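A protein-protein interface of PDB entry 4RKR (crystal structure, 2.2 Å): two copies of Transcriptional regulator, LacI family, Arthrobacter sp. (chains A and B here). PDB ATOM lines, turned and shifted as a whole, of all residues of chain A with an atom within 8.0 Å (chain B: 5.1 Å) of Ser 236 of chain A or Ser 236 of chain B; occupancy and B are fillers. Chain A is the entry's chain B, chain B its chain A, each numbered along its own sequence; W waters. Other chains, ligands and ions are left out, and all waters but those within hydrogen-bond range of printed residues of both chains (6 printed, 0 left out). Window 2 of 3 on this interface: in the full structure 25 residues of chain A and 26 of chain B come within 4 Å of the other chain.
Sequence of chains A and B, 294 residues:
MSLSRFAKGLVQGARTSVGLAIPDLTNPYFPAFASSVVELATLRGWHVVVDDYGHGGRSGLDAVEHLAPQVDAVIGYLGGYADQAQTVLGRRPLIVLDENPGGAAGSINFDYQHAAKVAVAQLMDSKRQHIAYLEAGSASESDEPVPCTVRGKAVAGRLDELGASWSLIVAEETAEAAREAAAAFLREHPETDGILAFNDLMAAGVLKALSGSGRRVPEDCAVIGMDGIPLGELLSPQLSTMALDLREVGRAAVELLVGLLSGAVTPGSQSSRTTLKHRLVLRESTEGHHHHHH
The backbone NH of Gln 238 of chain A sits at hydrogen-bond distance from the side-chain carboxylate of Glu 284 of chain A (2.9 Å).
O of Gln 238 of chain A sits at hydrogen-bond distance from N of Ser 285 of chain A (2.9 Å).
The backbone NH (N) of Gln 238 of chain B lies within hydrogen-bond range of the side-chain carboxylate (OE1) of Glu 284 of chain B, 3.0 Å away.
NZ of Lys 208 of chain A touches O of Leu 234 of chain B (3.9 Å).
NZ of Lys 208 of chain A touches CB of Ser 236 of chain B, 3.3 Å away.
Lys 208 of chain A touches Gln 238 of chain B (CE to CG, 3.9 Å).
Lys 208 of chain B touches Glu 233 of chain A (CE to O, 3.2 Å).
Leu 234 of chain A touches Lys 208 of chain B (O to NZ, 3.8 Å).
O of Leu 234 of chain A touches CD2 of Leu 235 of chain B, at 3.5 Å.
Leu 234 of chain B touches Leu 235 of chain A (O to CD2, 3.6 Å).
Ser 236 of chain B touches Ser 236 of chain A (CB to O, 3.5 Å).
Lys 208 of chain B touches Gln 238 of chain A.
Printed residues of chain B that touch a printed residue of chain A: Lys 208, Leu 234, Leu 235, Ser 236 and Gln 238.
Along chain B the printed residues that touch a printed residue of chain A span positions 208 to 238.
Printed residues of chain A that touch a printed residue of chain B: Lys 208, Glu 233, Leu 234, Leu 235, Ser 236 and Gln 238.
Hydrophobic or aromatic side chains of chain A that line the printed part of chain B: Leu 235.
Among the printed residues, no Asp or Glu carboxylate lies within 4 Å of a Lys or Arg side-chain nitrogen of the other chain.
Ser 236 of chain A touches just one residue of chain B: Ser 236 (3.5 Å).
Ser 236 of chain B touches just these residues of chain A: Lys 208 (3.3 Å) and Ser 236 (3.5 Å).
No residue of chain A comes within 4 Å of Pro 237 of chain B.
Printed residues of chain A within 4 Å of Leu 235 of chain B: Lys 208 and Leu 234.
Of the printed residues of chain B, Leu 234 of chain A touches Lys 208 (3.8 Å) and Leu 235 (3.5 Å).
Printed residues of chain A within 4 Å of Leu 234 of chain B: Lys 208 and Leu 235.
Of the printed residues of chain B, Leu 235 of chain A touches Lys 208 and Leu 234.
Of the printed residues of chain B, Glu 233 of chain A touches Lys 208 (3.2 Å).
Ser 211 of chain A touches none of the printed residues of chain B.
Ala 204 of chain A touches none of the printed residues of chain B.
Water W3 lies within hydrogen-bond range of OE1 of Glu 284 of chain B (2.5 Å), OG of Ser 236 of chain B (2.6 Å) and NZ of Lys 208 of chain A (2.6 Å).
Water W6 lies within hydrogen-bond range of OE2 of Glu 284 of chain A (2.7 Å), NZ of Lys 208 of chain B (3.0 Å) and OE1 of Gln 238 of chain A (3.3 Å).
Water W1 lies within hydrogen-bond range of the backbone carbonyl oxygen of Ala 204 of chain A (2.7 Å) and the backbone carbonyl oxygen of Leu 234 of chain B (2.9 Å).
Water W2 lies within hydrogen-bond range of O of Leu 234 of chain A (2.8 Å), N of Ser 236 of chain B (2.9 Å) and N of Ser 236 of chain A (3.4 Å).
Water W4 lies within hydrogen-bond range of OE2 of Glu 284 of chain B (2.8 Å), NZ of Lys 208 of chain A (3.2 Å) and OE1 of Gln 238 of chain B (3.3 Å).
Water W5 lies within hydrogen-bond range of the backbone carbonyl oxygen of Leu 234 of chain B (2.9 Å), the backbone NH of Ser 236 of chain A (3.0 Å) and the backbone NH of Ser 236 of chain B (3.2 Å).
Lys 208 of chain A touches Leu 234 of chain B, and with the chains exchanged Leu 234 of chain A touches Lys 208 of chain B.
Lys 208 of chain A touches Ser 236 of chain B, but with the chains exchanged Ser 236 of chain A does not touch Lys 208 of chain B (4.1 Å).
Lys 208 of chain A touches Gln 238 of chain B, and with the chains exchanged Gln 238 of chain A touches Lys 208 of chain B.
Ser 236 of chain B touches its own counterpart, Ser 236 of chain A.
8 positions are printed for both chains.
The backbone carbonyl oxygen (O) of Leu 235 of chain A lies within hydrogen-bond range of the side-chain amino group (NZ) of Lys 208 of chain B, at 3.1 Å.
The backbone carbonyl oxygen (O) of Leu 235 of chain B is in hydrogen-bond range of the side-chain amino group (NZ) of Lys 208 of chain A (2.6 Å).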
ATOM      1  N   ALA A 204      30.805  17.208  -3.582  1.00  0.00           N
ATOM      2  CA  ALA A 204      30.965  15.749  -3.545  1.00  0.00           C
ATOM      3  C   ALA A 204      32.291  15.366  -2.904  1.00  0.00           C
ATOM      4  O   ALA A 204      32.372  14.393  -2.162  1.00  0.00           O
ATOM      5  CB  ALA A 204      30.890  15.174  -4.943  1.00  0.00           C
ATOM      6  N   LEU A 207      31.971  15.901   1.006  1.00  0.00           N
ATOM      7  CA  LEU A 207      31.304  14.740   1.603  1.00  0.00           C
ATOM      8  C   LEU A 207      32.255  13.589   1.860  1.00  0.00           C
ATOM      9  O   LEU A 207      32.150  12.897   2.881  1.00  0.00           O
ATOM     10  CB  LEU A 207      30.186  14.224   0.701  1.00  0.00           C
ATOM     11  CG  LEU A 207      28.934  15.077   0.564  1.00  0.00           C
ATOM     12  CD1 LEU A 207      27.965  14.429  -0.425  1.00  0.00           C
ATOM     13  CD2 LEU A 207      28.281  15.280   1.920  1.00  0.00           C
ATOM     14  N   LYS A 208      33.169  13.377   0.920  1.00  0.00           N
ATOM     15  CA  LYS A 208      34.123  12.284   1.022  1.00  0.00           C
ATOM     16  C   LYS A 208      35.134  12.547   2.116  1.00  0.00           C
ATOM     17  O   LYS A 208      35.527  11.623   2.818  1.00  0.00           O
ATOM     18  CB  LYS A 208      34.828  12.028  -0.316  1.00  0.00           C
ATOM     19  CG  LYS A 208      34.911  10.557  -0.680  1.00  0.00           C
ATOM     20  CD  LYS A 208      33.524   9.924  -0.673  1.00  0.00           C
ATOM     21  CE  LYS A 208      33.503   8.581  -1.373  1.00  0.00           C
ATOM     22  NZ  LYS A 208      32.291   7.818  -0.992  1.00  0.00           N
ATOM     23  N   SER A 211      33.186  11.847   5.344  1.00  0.00           N
ATOM     24  CA  SER A 211      33.154  10.382   5.412  1.00  0.00           C
ATOM     25  C   SER A 211      34.467   9.788   5.937  1.00  0.00           C
ATOM     26  O   SER A 211      34.477   9.038   6.921  1.00  0.00           O
ATOM     27  CB  SER A 211      32.853   9.805   4.025  1.00  0.00           C
ATOM     28  OG  SER A 211      33.273   8.461   3.925  1.00  0.00           O
ATOM     29  N   VAL A 217      26.983  12.884   8.353  1.00  0.00           N
ATOM     30  CA  VAL A 217      26.338  14.004   7.663  1.00  0.00           C
ATOM     31  C   VAL A 217      24.838  13.711   7.603  1.00  0.00           C
ATOM     32  O   VAL A 217      24.446  12.633   7.121  1.00  0.00           O
ATOM     33  CB  VAL A 217      26.936  14.185   6.245  1.00  0.00           C
ATOM     34  CG1 VAL A 217      26.208  15.266   5.456  1.00  0.00           C
ATOM     35  CG2 VAL A 217      28.428  14.487   6.340  1.00  0.00           C
ATOM     36  N   LEU A 231      24.052  14.204 -10.416  1.00  0.00           N
ATOM     37  CA  LEU A 231      24.972  13.579  -9.471  1.00  0.00           C
ATOM     38  C   LEU A 231      24.544  13.663  -7.995  1.00  0.00           C
ATOM     39  O   LEU A 231      24.758  12.717  -7.221  1.00  0.00           O
ATOM     40  CB  LEU A 231      26.339  14.264  -9.645  1.00  0.00           C
ATOM     41  CG  LEU A 231      27.481  13.885  -8.729  1.00  0.00           C
ATOM     42  CD1 LEU A 231      27.802  12.428  -8.961  1.00  0.00           C
ATOM     43  CD2 LEU A 231      28.697  14.756  -8.988  1.00  0.00           C
ATOM     44  N   GLY A 232      23.964  14.800  -7.606  1.00  0.00           N
ATOM     45  CA  GLY A 232      23.564  15.051  -6.218  1.00  0.00           C
ATOM     46  C   GLY A 232      22.614  14.010  -5.663  1.00  0.00           C
ATOM     47  O   GLY A 232      22.695  13.647  -4.490  1.00  0.00           O
ATOM     48  N   GLU A 233      21.729  13.511  -6.521  1.00  0.00           N
ATOM     49  CA  GLU A 233      20.767  12.477  -6.133  1.00  0.00           C
ATOM     50  C   GLU A 233      21.372  11.077  -6.032  1.00  0.00           C
ATOM     51  O   GLU A 233      20.717  10.160  -5.545  1.00  0.00           O
ATOM     52  CB  GLU A 233      19.578  12.473  -7.105  1.00  0.00           C
ATOM     53  CG  GLU A 233      18.750  13.748  -7.014  1.00  0.00           C
ATOM     54  CD  GLU A 233      17.578  13.780  -7.973  1.00  0.00           C
ATOM     55  OE1 GLU A 233      17.423  12.829  -8.761  1.00  0.00           O
ATOM     56  OE2 GLU A 233      16.811  14.768  -7.943  1.00  0.00           O
ATOM     57  N   LEU A 234      22.605  10.900  -6.490  1.00  0.00           N
ATOM     58  CA  LEU A 234      23.248   9.588  -6.450  1.00  0.00           C
ATOM     59  C   LEU A 234      24.245   9.483  -5.344  1.00  0.00           C
ATOM     60  O   LEU A 234      24.682   8.385  -5.015  1.00  0.00           O
ATOM     61  CB  LEU A 234      23.939   9.296  -7.780  1.00  0.00           C
ATOM     62  CG  LEU A 234      22.988   9.342  -8.981  1.00  0.00           C
ATOM     63  CD1 LEU A 234      23.737   9.164 -10.295  1.00  0.00           C
ATOM     64  CD2 LEU A 234      21.902   8.295  -8.838  1.00  0.00           C
ATOM     65  N   LEU A 235      24.611  10.622  -4.769  1.00  0.00           N
ATOM     66  CA  LEU A 235      25.531  10.630  -3.658  1.00  0.00           C
ATOM     67  C   LEU A 235      24.847  10.069  -2.431  1.00  0.00           C
ATOM     68  O   LEU A 235      23.621  10.031  -2.358  1.00  0.00           O
ATOM     69  CB  LEU A 235      26.025  12.049  -3.384  1.00  0.00           C
ATOM     70  CG  LEU A 235      26.756  12.698  -4.566  1.00  0.00           C
ATOM     71  CD1 LEU A 235      27.198  14.114  -4.240  1.00  0.00           C
ATOM     72  CD2 LEU A 235      27.948  11.856  -4.991  1.00  0.00           C
ATOM     73  N   SER A 236      25.652   9.613  -1.481  1.00  0.00           N
ATOM     74  CA  SER A 236      25.149   9.206  -0.176  1.00  0.00           C
ATOM     75  C   SER A 236      26.004   9.843   0.915  1.00  0.00           C
ATOM     76  O   SER A 236      27.165   9.467   1.069  1.00  0.00           O
ATOM     77  CB  SER A 236      25.191   7.694  -0.033  1.00  0.00           C
ATOM     78  OG  SER A 236      24.621   7.320   1.205  1.00  0.00           O
ATOM     79  N   PRO A 237      25.455  10.795   1.673  1.00  0.00           N
ATOM     80  CA  PRO A 237      24.052  11.237   1.571  1.00  0.00           C
ATOM     81  C   PRO A 237      23.778  12.054   0.327  1.00  0.00           C
ATOM     82  O   PRO A 237      24.674  12.725  -0.181  1.00  0.00           O
ATOM     83  CB  PRO A 237      23.881  12.135   2.794  1.00  0.00           C
ATOM     84  CG  PRO A 237      25.249  12.685   3.024  1.00  0.00           C
ATOM     85  CD  PRO A 237      26.208  11.587   2.661  1.00  0.00           C
ATOM     86  N   GLN A 238      22.543  11.998  -0.152  1.00  0.00           N
ATOM     87  CA  GLN A 238      22.118  12.862  -1.232  1.00  0.00           C
ATOM     88  C   GLN A 238      22.375  14.310  -0.827  1.00  0.00           C
ATOM     89  O   GLN A 238      22.306  14.652   0.349  1.00  0.00           O
ATOM     90  CB  GLN A 238      20.657  12.610  -1.579  1.00  0.00           C
ATOM     91  CG  GLN A 238      20.444  11.252  -2.239  1.00  0.00           C
ATOM     92  CD  GLN A 238      19.026  11.040  -2.741  1.00  0.00           C
ATOM     93  OE1 GLN A 238      18.477   9.955  -2.633  1.00  0.00           O
ATOM     94  NE2 GLN A 238      18.439  12.065  -3.295  1.00  0.00           N
ATOM     95  N   LEU A 239      22.702  15.143  -1.810  1.00  0.00           N
ATOM     96  CA  LEU A 239      23.305  16.446  -1.562  1.00  0.00           C
ATOM     97  C   LEU A 239      22.298  17.583  -1.685  1.00  0.00           C
ATOM     98  O   LEU A 239      21.685  17.765  -2.724  1.00  0.00           O
ATOM     99  CB  LEU A 239      24.472  16.667  -2.539  1.00  0.00           C
ATOM    100  CG  LEU A 239      25.053  18.077  -2.687  1.00  0.00           C
ATOM    101  CD1 LEU A 239      25.812  18.499  -1.439  1.00  0.00           C
ATOM    102  CD2 LEU A 239      25.943  18.162  -3.923  1.00  0.00           C
ATOM    103  N   GLU A 284      19.437  14.799   1.832  1.00  0.00           N
ATOM    104  CA  GLU A 284      20.027  14.227   3.032  1.00  0.00           C
ATOM    105  C   GLU A 284      21.201  14.965   3.666  1.00  0.00           C
ATOM    106  O   GLU A 284      21.539  14.689   4.798  1.00  0.00           O
ATOM    107  CB  GLU A 284      20.435  12.791   2.770  1.00  0.00           C
ATOM    108  CG  GLU A 284      19.324  11.928   2.230  1.00  0.00           C
ATOM    109  CD  GLU A 284      19.840  10.655   1.613  1.00  0.00           C
ATOM    110  OE1 GLU A 284      21.047  10.386   1.699  1.00  0.00           O
ATOM    111  OE2 GLU A 284      19.027   9.916   1.041  1.00  0.00           O
ATOM    112  N   SER A 285      21.882  15.821   2.925  1.00  0.00           N
ATOM    113  CA  SER A 285      23.137  16.411   3.431  1.00  0.00           C
ATOM    114  C   SER A 285      22.879  17.561   4.407  1.00  0.00           C
ATOM    115  O   SER A 285      23.826  18.092   4.972  1.00  0.00           O
ATOM    116  CB  SER A 285      24.047  16.886   2.286  1.00  0.00           C
ATOM    117  OG  SER A 285      23.524  18.026   1.620  1.00  0.00           O
ATOM    118  N   LEU B 207      23.131   0.685  -6.057  1.00  0.00           N
ATOM    119  CA  LEU B 207      23.587   1.072  -4.728  1.00  0.00           C
ATOM    120  C   LEU B 207      22.449   1.732  -3.944  1.00  0.00           C
ATOM    121  O   LEU B 207      22.222   1.380  -2.796  1.00  0.00           O
ATOM    122  CB  LEU B 207      24.816   1.983  -4.802  1.00  0.00           C
ATOM    123  CG  LEU B 207      26.111   1.340  -5.316  1.00  0.00           C
ATOM    124  CD1 LEU B 207      27.247   2.349  -5.342  1.00  0.00           C
ATOM    125  CD2 LEU B 207      26.520   0.143  -4.469  1.00  0.00           C
ATOM    126  N   LYS B 208      21.710   2.646  -4.578  1.00  0.00           N
ATOM    127  CA  LYS B 208      20.574   3.325  -3.924  1.00  0.00           C
ATOM    128  C   LYS B 208      19.517   2.360  -3.438  1.00  0.00           C
ATOM    129  O   LYS B 208      18.975   2.532  -2.343  1.00  0.00           O
ATOM    130  CB  LYS B 208      19.882   4.329  -4.870  1.00  0.00           C
ATOM    131  CG  LYS B 208      20.470   5.723  -4.868  1.00  0.00           C
ATOM    132  CD  LYS B 208      19.969   6.531  -3.688  1.00  0.00           C
ATOM    133  CE  LYS B 208      20.853   7.739  -3.441  1.00  0.00           C
ATOM    134  NZ  LYS B 208      21.980   7.402  -2.537  1.00  0.00           N
ATOM    135  N   LEU B 234      33.245   8.891  -6.352  1.00  0.00           N
ATOM    136  CA  LEU B 234      32.481   9.824  -5.533  1.00  0.00           C
ATOM    137  C   LEU B 234      31.263   9.188  -4.864  1.00  0.00           C
ATOM    138  O   LEU B 234      30.697   9.761  -3.937  1.00  0.00           O
ATOM    139  CB  LEU B 234      32.022  11.006  -6.400  1.00  0.00           C
ATOM    140  CG  LEU B 234      33.120  11.742  -7.182  1.00  0.00           C
ATOM    141  CD1 LEU B 234      32.531  12.895  -7.982  1.00  0.00           C
ATOM    142  CD2 LEU B 234      34.217  12.250  -6.254  1.00  0.00           C
ATOM    143  N   LEU B 235      30.831   8.028  -5.349  1.00  0.00           N
ATOM    144  CA  LEU B 235      29.714   7.329  -4.726  1.00  0.00           C
ATOM    145  C   LEU B 235      30.167   6.794  -3.381  1.00  0.00           C
ATOM    146  O   LEU B 235      31.365   6.659  -3.148  1.00  0.00           O
ATOM    147  CB  LEU B 235      29.256   6.163  -5.594  1.00  0.00           C
ATOM    148  CG  LEU B 235      28.711   6.503  -6.984  1.00  0.00           C
ATOM    149  CD1 LEU B 235      28.373   5.220  -7.723  1.00  0.00           C
ATOM    150  CD2 LEU B 235      27.481   7.395  -6.905  1.00  0.00           C
ATOM    151  N   SER B 236      29.208   6.507  -2.500  1.00  0.00           N
ATOM    152  CA  SER B 236      29.485   5.866  -1.217  1.00  0.00           C
ATOM    153  C   SER B 236      28.541   4.688  -1.062  1.00  0.00           C
ATOM    154  O   SER B 236      27.337   4.895  -0.999  1.00  0.00           O
ATOM    155  CB  SER B 236      29.277   6.852  -0.069  1.00  0.00           C
ATOM    156  OG  SER B 236      29.829   6.333   1.124  1.00  0.00           O
ATOM    157  N   PRO B 237      29.045   3.451  -1.039  1.00  0.00           N
ATOM    158  CA  PRO B 237      30.461   3.134  -1.188  1.00  0.00           C
ATOM    159  C   PRO B 237      30.986   3.420  -2.595  1.00  0.00           C
ATOM    160  O   PRO B 237      30.205   3.455  -3.549  1.00  0.00           O
ATOM    161  CB  PRO B 237      30.502   1.635  -0.898  1.00  0.00           C
ATOM    162  CG  PRO B 237      29.162   1.145  -1.348  1.00  0.00           C
ATOM    163  CD  PRO B 237      28.214   2.236  -0.962  1.00  0.00           C
ATOM    164  N   GLN B 238      32.292   3.659  -2.702  1.00  0.00           N
ATOM    165  CA  GLN B 238      32.951   3.795  -3.993  1.00  0.00           C
ATOM    166  C   GLN B 238      32.735   2.515  -4.798  1.00  0.00           C
ATOM    167  O   GLN B 238      32.726   1.411  -4.257  1.00  0.00           O
ATOM    168  CB  GLN B 238      34.443   4.069  -3.812  1.00  0.00           C
ATOM    169  CG  GLN B 238      34.754   5.468  -3.308  1.00  0.00           C
ATOM    170  CD  GLN B 238      36.240   5.761  -3.271  1.00  0.00           C
ATOM    171  OE1 GLN B 238      36.784   6.129  -2.238  1.00  0.00           O
ATOM    172  NE2 GLN B 238      36.900   5.598  -4.396  1.00  0.00           N
ATOM    173  N   GLU B 284      35.349   0.174  -2.910  1.00  0.00           N
ATOM    174  CA  GLU B 284      34.552  -0.213  -1.752  1.00  0.00           C
ATOM    175  C   GLU B 284      33.420  -1.235  -1.929  1.00  0.00           C
ATOM    176  O   GLU B 284      33.060  -1.897  -0.984  1.00  0.00           O
ATOM    177  CB  GLU B 284      34.060   1.032  -1.018  1.00  0.00           C
ATOM    178  CG  GLU B 284      35.197   1.900  -0.517  1.00  0.00           C
ATOM    179  CD  GLU B 284      34.731   3.171   0.150  1.00  0.00           C
ATOM    180  OE1 GLU B 284      33.543   3.507   0.030  1.00  0.00           O
ATOM    181  OE2 GLU B 284      35.561   3.828   0.802  1.00  0.00           O
HETATM  182  O   HOH W   1      30.920  12.120  -2.318  1.00  0.00           O
HETATM  183  O   HOH W   2      26.523   7.033  -3.446  1.00  0.00           O
HETATM  184  O   HOH W   3      32.195   5.592   0.441  1.00  0.00           O
HETATM  185  O   HOH W   4      34.905   6.517   0.408  1.00  0.00           O
HETATM  186  O   HOH W   5      28.641   9.554  -1.937  1.00  0.00           O
HETATM  187  O   HOH W   6      19.878   7.876  -0.466  1.00  0.00           O
